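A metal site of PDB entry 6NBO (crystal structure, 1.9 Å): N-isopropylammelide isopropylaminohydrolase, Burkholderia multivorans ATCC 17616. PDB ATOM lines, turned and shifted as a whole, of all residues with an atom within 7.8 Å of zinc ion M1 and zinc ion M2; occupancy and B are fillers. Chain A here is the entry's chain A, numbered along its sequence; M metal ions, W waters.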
ATOM      1  N   HIS A  65      16.983 -11.238   0.639  1.00  0.00           N
ATOM      2  CA  HIS A  65      16.336 -10.407   1.663  1.00  0.00           C
ATOM      3  C   HIS A  65      14.832 -10.382   1.418  1.00  0.00           C
ATOM      4  O   HIS A  65      14.355  -9.664   0.546  1.00  0.00           O
ATOM      5  CB  HIS A  65      16.873  -8.973   1.673  1.00  0.00           C
ATOM      6  CG  HIS A  65      16.336  -8.098   2.777  1.00  0.00           C
ATOM      7  ND1 HIS A  65      17.153  -7.497   3.717  1.00  0.00           N
ATOM      8  CD2 HIS A  65      15.077  -7.662   3.046  1.00  0.00           C
ATOM      9  CE1 HIS A  65      16.413  -6.749   4.527  1.00  0.00           C
ATOM     10  NE2 HIS A  65      15.153  -6.847   4.145  1.00  0.00           N
ATOM     11  N   THR A  66      14.082 -11.156   2.181  1.00  0.00           N
ATOM     12  CA  THR A  66      12.637 -11.002   2.168  1.00  0.00           C
ATOM     13  C   THR A  66      12.132 -11.171   3.606  1.00  0.00           C
ATOM     14  O   THR A  66      12.922 -11.291   4.553  1.00  0.00           O
ATOM     15  CB  THR A  66      11.987 -11.971   1.177  1.00  0.00           C
ATOM     16  OG1 THR A  66      10.606 -11.596   1.000  1.00  0.00           O
ATOM     17  CG2 THR A  66      12.064 -13.431   1.674  1.00  0.00           C
ATOM     18  N   HIS A  67      10.801 -11.173   3.756  1.00  0.00           N
ATOM     19  CA  HIS A  67      10.126 -11.237   5.050  1.00  0.00           C
ATOM     20  C   HIS A  67       8.995 -12.258   4.875  1.00  0.00           C
ATOM     21  O   HIS A  67       7.840 -11.874   4.695  1.00  0.00           O
ATOM     22  CB  HIS A  67       9.603  -9.864   5.503  1.00  0.00           C
ATOM     23  CG  HIS A  67      10.676  -8.857   5.784  1.00  0.00           C
ATOM     24  ND1 HIS A  67      11.197  -8.666   7.053  1.00  0.00           N
ATOM     25  CD2 HIS A  67      11.335  -7.988   4.982  1.00  0.00           C
ATOM     26  CE1 HIS A  67      12.106  -7.712   7.012  1.00  0.00           C
ATOM     27  NE2 HIS A  67      12.221  -7.288   5.767  1.00  0.00           N
ATOM     28  N   LYS A  70       5.687 -12.154   6.952  1.00  0.00           N
ATOM     29  CA  LYS A  70       4.741 -11.049   6.812  1.00  0.00           C
ATOM     30  C   LYS A  70       3.807 -11.183   5.611  1.00  0.00           C
ATOM     31  O   LYS A  70       2.794 -10.477   5.549  1.00  0.00           O
ATOM     32  CB  LYS A  70       5.471  -9.708   6.640  1.00  0.00           C
ATOM     33  CG  LYS A  70       6.358  -9.194   7.774  1.00  0.00           C
ATOM     34  CD  LYS A  70       7.029  -7.901   7.287  1.00  0.00           C
ATOM     35  CE  LYS A  70       8.140  -7.403   8.215  1.00  0.00           C
ATOM     36  NZ  LYS A  70       7.627  -6.815   9.480  1.00  0.00           N
ATOM     37  N   HIS A 126      14.168 -12.434   6.870  1.00  0.00           N
ATOM     38  CA  HIS A 126      14.020 -11.883   8.197  1.00  0.00           C
ATOM     39  C   HIS A 126      12.684 -12.335   8.749  1.00  0.00           C
ATOM     40  O   HIS A 126      11.751 -12.622   7.992  1.00  0.00           O
ATOM     41  CB  HIS A 126      14.125 -10.360   8.126  1.00  0.00           C
ATOM     42  CG  HIS A 126      15.449  -9.895   7.559  1.00  0.00           C
ATOM     43  ND1 HIS A 126      16.396  -9.251   8.318  1.00  0.00           N
ATOM     44  CD2 HIS A 126      15.976 -10.032   6.329  1.00  0.00           C
ATOM     45  CE1 HIS A 126      17.461  -9.006   7.580  1.00  0.00           C
ATOM     46  NE2 HIS A 126      17.234  -9.465   6.364  1.00  0.00           N
ATOM     47  N   PHE A 159      14.622 -10.713  13.613  1.00  0.00           N
ATOM     48  CA  PHE A 159      14.526  -9.272  13.336  1.00  0.00           C
ATOM     49  C   PHE A 159      13.640  -8.546  14.353  1.00  0.00           C
ATOM     50  O   PHE A 159      12.403  -8.695  14.313  1.00  0.00           O
ATOM     51  CB  PHE A 159      13.978  -9.069  11.913  1.00  0.00           C
ATOM     52  CG  PHE A 159      13.809  -7.629  11.491  1.00  0.00           C
ATOM     53  CD1 PHE A 159      14.865  -6.724  11.635  1.00  0.00           C
ATOM     54  CD2 PHE A 159      12.616  -7.192  10.927  1.00  0.00           C
ATOM     55  CE1 PHE A 159      14.721  -5.402  11.242  1.00  0.00           C
ATOM     56  CE2 PHE A 159      12.471  -5.869  10.534  1.00  0.00           C
ATOM     57  CZ  PHE A 159      13.526  -4.962  10.702  1.00  0.00           C
ATOM     58  N   GLN A 161      11.728  -5.980  14.811  1.00  0.00           N
ATOM     59  CA  GLN A 161      11.192  -4.986  13.880  1.00  0.00           C
ATOM     60  C   GLN A 161      10.870  -3.665  14.575  1.00  0.00           C
ATOM     61  O   GLN A 161      11.046  -2.595  13.980  1.00  0.00           O
ATOM     62  CB  GLN A 161       9.958  -5.545  13.169  1.00  0.00           C
ATOM     63  CG  GLN A 161       9.051  -4.514  12.481  1.00  0.00           C
ATOM     64  CD  GLN A 161       9.589  -4.039  11.150  1.00  0.00           C
ATOM     65  OE1 GLN A 161       9.236  -4.570  10.092  1.00  0.00           O
ATOM     66  NE2 GLN A 161      10.447  -3.018  11.184  1.00  0.00           N
ATOM     67  N   ASP A 216      22.673  -9.322  10.243  1.00  0.00           N
ATOM     68  CA  ASP A 216      22.197  -8.668   9.024  1.00  0.00           C
ATOM     69  C   ASP A 216      21.293  -7.542   9.495  1.00  0.00           C
ATOM     70  O   ASP A 216      20.196  -7.793   9.988  1.00  0.00           O
ATOM     71  CB  ASP A 216      21.446  -9.654   8.111  1.00  0.00           C
ATOM     72  CG  ASP A 216      20.996  -9.043   6.788  1.00  0.00           C
ATOM     73  OD1 ASP A 216      20.680  -7.837   6.752  1.00  0.00           O
ATOM     74  OD2 ASP A 216      20.968  -9.775   5.776  1.00  0.00           O
ATOM     75  N   HIS A 218      19.183  -3.955   9.165  1.00  0.00           N
ATOM     76  CA  HIS A 218      18.473  -2.971   8.351  1.00  0.00           C
ATOM     77  C   HIS A 218      19.005  -1.573   8.670  1.00  0.00           C
ATOM     78  O   HIS A 218      18.935  -1.131   9.818  1.00  0.00           O
ATOM     79  CB  HIS A 218      16.966  -2.995   8.656  1.00  0.00           C
ATOM     80  CG  HIS A 218      16.214  -4.139   8.027  1.00  0.00           C
ATOM     81  ND1 HIS A 218      16.430  -5.450   8.390  1.00  0.00           N
ATOM     82  CD2 HIS A 218      15.219  -4.154   7.108  1.00  0.00           C
ATOM     83  CE1 HIS A 218      15.606  -6.229   7.702  1.00  0.00           C
ATOM     84  NE2 HIS A 218      14.862  -5.462   6.913  1.00  0.00           N
ATOM     85  N   HIS A 220      18.122   2.004   7.360  1.00  0.00           N
ATOM     86  CA  HIS A 220      17.372   2.955   6.560  1.00  0.00           C
ATOM     87  C   HIS A 220      17.837   4.388   6.751  1.00  0.00           C
ATOM     88  O   HIS A 220      17.392   5.264   6.005  1.00  0.00           O
ATOM     89  CB  HIS A 220      15.886   2.952   6.905  1.00  0.00           C
ATOM     90  CG  HIS A 220      15.274   1.584   6.998  1.00  0.00           C
ATOM     91  ND1 HIS A 220      15.133   0.910   8.194  1.00  0.00           N
ATOM     92  CD2 HIS A 220      14.743   0.790   6.047  1.00  0.00           C
ATOM     93  CE1 HIS A 220      14.540  -0.247   7.968  1.00  0.00           C
ATOM     94  NE2 HIS A 220      14.298  -0.352   6.679  1.00  0.00           N
ATOM     95  N   SER A 249      21.677  -4.216   5.259  1.00  0.00           N
ATOM     96  CA  SER A 249      20.547  -4.199   4.335  1.00  0.00           C
ATOM     97  C   SER A 249      20.088  -2.769   4.084  1.00  0.00           C
ATOM     98  O   SER A 249      20.012  -1.966   5.014  1.00  0.00           O
ATOM     99  CB  SER A 249      19.384  -5.041   4.881  1.00  0.00           C
ATOM    100  OG  SER A 249      19.652  -6.439   4.744  1.00  0.00           O
ATOM    101  N   HIS A 250      19.752  -2.494   2.815  1.00  0.00           N
ATOM    102  CA  HIS A 250      19.213  -1.229   2.308  1.00  0.00           C
ATOM    103  C   HIS A 250      20.330  -0.197   2.143  1.00  0.00           C
ATOM    104  O   HIS A 250      20.721   0.105   1.014  1.00  0.00           O
ATOM    105  CB  HIS A 250      18.070  -0.728   3.195  1.00  0.00           C
ATOM    106  CG  HIS A 250      16.971  -1.730   3.349  1.00  0.00           C
ATOM    107  ND1 HIS A 250      16.468  -2.456   2.280  1.00  0.00           N
ATOM    108  CD2 HIS A 250      16.303  -2.176   4.435  1.00  0.00           C
ATOM    109  CE1 HIS A 250      15.528  -3.276   2.706  1.00  0.00           C
ATOM    110  NE2 HIS A 250      15.403  -3.116   4.010  1.00  0.00           N
ATOM    111  N   PHE A 252      20.614   2.985   2.400  1.00  0.00           N
ATOM    112  CA  PHE A 252      20.258   4.131   1.577  1.00  0.00           C
ATOM    113  C   PHE A 252      21.271   5.274   1.709  1.00  0.00           C
ATOM    114  O   PHE A 252      21.471   6.040   0.749  1.00  0.00           O
ATOM    115  CB  PHE A 252      18.876   4.658   1.946  1.00  0.00           C
ATOM    116  CG  PHE A 252      17.788   3.620   1.879  1.00  0.00           C
ATOM    117  CD1 PHE A 252      17.784   2.661   0.876  1.00  0.00           C
ATOM    118  CD2 PHE A 252      16.764   3.622   2.807  1.00  0.00           C
ATOM    119  CE1 PHE A 252      16.776   1.709   0.824  1.00  0.00           C
ATOM    120  CE2 PHE A 252      15.760   2.679   2.758  1.00  0.00           C
ATOM    121  CZ  PHE A 252      15.760   1.727   1.759  1.00  0.00           C
ATOM    122  N   VAL A 277      22.833  -5.393   0.894  1.00  0.00           N
ATOM    123  CA  VAL A 277      21.602  -5.851   0.254  1.00  0.00           C
ATOM    124  C   VAL A 277      20.910  -4.639  -0.352  1.00  0.00           C
ATOM    125  O   VAL A 277      20.697  -3.639   0.337  1.00  0.00           O
ATOM    126  CB  VAL A 277      20.663  -6.546   1.258  1.00  0.00           C
ATOM    127  CG1 VAL A 277      19.319  -6.802   0.602  1.00  0.00           C
ATOM    128  CG2 VAL A 277      21.295  -7.815   1.781  1.00  0.00           C
ATOM    129  N   THR A 279      17.316  -3.739  -2.542  1.00  0.00           N
ATOM    130  CA  THR A 279      16.053  -4.195  -3.119  1.00  0.00           C
ATOM    131  C   THR A 279      15.575  -3.243  -4.193  1.00  0.00           C
ATOM    132  O   THR A 279      14.448  -3.381  -4.697  1.00  0.00           O
ATOM    133  CB  THR A 279      15.019  -4.364  -2.013  1.00  0.00           C
ATOM    134  OG1 THR A 279      14.654  -3.081  -1.496  1.00  0.00           O
ATOM    135  CG2 THR A 279      15.599  -5.230  -0.892  1.00  0.00           C
ATOM    136  N   ASN A 303      13.878  -8.949  -2.623  1.00  0.00           N
ATOM    137  CA  ASN A 303      12.584  -8.297  -2.828  1.00  0.00           C
ATOM    138  C   ASN A 303      12.251  -7.304  -1.738  1.00  0.00           C
ATOM    139  O   ASN A 303      11.568  -6.313  -2.002  1.00  0.00           O
ATOM    140  CB  ASN A 303      11.438  -9.325  -2.881  1.00  0.00           C
ATOM    141  CG  ASN A 303      11.252  -9.935  -4.244  1.00  0.00           C
ATOM    142  OD1 ASN A 303      10.667  -9.329  -5.150  1.00  0.00           O
ATOM    143  ND2 ASN A 303      11.751 -11.169  -4.423  1.00  0.00           N
ATOM    144  N   ASP A 304      12.712  -7.565  -0.507  1.00  0.00           N
ATOM    145  CA  ASP A 304      12.091  -7.047   0.710  1.00  0.00           C
ATOM    146  C   ASP A 304      10.721  -7.700   0.823  1.00  0.00           C
ATOM    147  O   ASP A 304      10.554  -8.867   0.458  1.00  0.00           O
ATOM    148  CB  ASP A 304      11.983  -5.515   0.726  1.00  0.00           C
ATOM    149  CG  ASP A 304      12.283  -4.939   2.097  1.00  0.00           C
ATOM    150  OD1 ASP A 304      12.588  -5.720   3.015  1.00  0.00           O
ATOM    151  OD2 ASP A 304      12.203  -3.701   2.259  1.00  0.00           O
ATOM    152  N   GLY A 305       9.717  -6.964   1.302  1.00  0.00           N
ATOM    153  CA  GLY A 305       8.404  -7.553   1.481  1.00  0.00           C
ATOM    154  C   GLY A 305       7.783  -8.018   0.165  1.00  0.00           C
ATOM    155  O   GLY A 305       8.098  -7.532  -0.917  1.00  0.00           O
ATOM    156  N   TRP A 310       2.880  -3.669   4.364  1.00  0.00           N
ATOM    157  CA  TRP A 310       3.749  -2.546   4.006  1.00  0.00           C
ATOM    158  C   TRP A 310       3.699  -2.252   2.514  1.00  0.00           C
ATOM    159  O   TRP A 310       3.613  -1.091   2.100  1.00  0.00           O
ATOM    160  CB  TRP A 310       5.202  -2.828   4.395  1.00  0.00           C
ATOM    161  CG  TRP A 310       5.530  -2.921   5.843  1.00  0.00           C
ATOM    162  CD1 TRP A 310       5.247  -3.965   6.684  1.00  0.00           C
ATOM    163  CD2 TRP A 310       6.248  -1.963   6.625  1.00  0.00           C
ATOM    164  NE1 TRP A 310       5.731  -3.704   7.937  1.00  0.00           N
ATOM    165  CE2 TRP A 310       6.346  -2.479   7.933  1.00  0.00           C
ATOM    166  CE3 TRP A 310       6.811  -0.712   6.350  1.00  0.00           C
ATOM    167  CZ2 TRP A 310       6.988  -1.792   8.959  1.00  0.00           C
ATOM    168  CZ3 TRP A 310       7.438  -0.026   7.367  1.00  0.00           C
ATOM    169  CH2 TRP A 310       7.524  -0.568   8.665  1.00  0.00           C
HETATM  170 ZN    ZN M   1      13.653  -5.714   5.007  1.00  0.00          ZN
HETATM  171 ZN    ZN M   2      12.575  -2.983   4.495  1.00  0.00          ZN
HETATM  172  O   HOH W   1      11.798  -4.237   6.269  1.00  0.00           O
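A ring nitrogen (ND1) of His 65 is in hydrogen-bond range of a ring nitrogen (NE2) of His 126 (3.3 Å).
The side-chain hydroxyl (OG1) of Thr 66 sits at hydrogen-bond distance from the backbone carbonyl oxygen (O) of Asp 304.
The backbone carbonyl oxygen (O) of His 65 sits at hydrogen-bond distance from the backbone NH (N) of Asn 303, 3.3 Å away.
The backbone carbonyl oxygen (O) of Val 277 sits at hydrogen-bond distance from the backbone NH (N) of His 250 (2.9 Å).
A ring nitrogen (ND1) of His 65 is in hydrogen-bond range of the side-chain hydroxyl of Ser 249, 2.9 Å away.
NE2 of His 250 touches zinc ion M1, at 3.3 Å.
Within 4 Å of zinc ion M1: His 65, His 67, His 218, His 250 and Asp 304.
His 220 touches zinc ion M2 (NE2 to ZN, 3.8 Å).
NE2 of His 250 touches zinc ion M2, at 2.9 Å.
Within 4 Å of zinc ion M2: His 218, His 220, His 250 and Asp 304.
The nearest printed residue that does not touch zinc ion M2 is His 67 (4.5 Å).
Zinc ion M1 is bound by NE2 of His 65 (2.1 Å), NE2 of His 67 (2.3 Å), OD1 of Asp 304 (2.3 Å) and NE2 of His 218 (2.3 Å).
Slightly farther from zinc ion M1 lies water W1 (2.7 Å).
Zinc ion M2 is bound by water W1, 2.3 Å away.
The side-chain carboxylate (OD2) of Asp 304 is bound to zinc ion M2 (2.4 Å).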
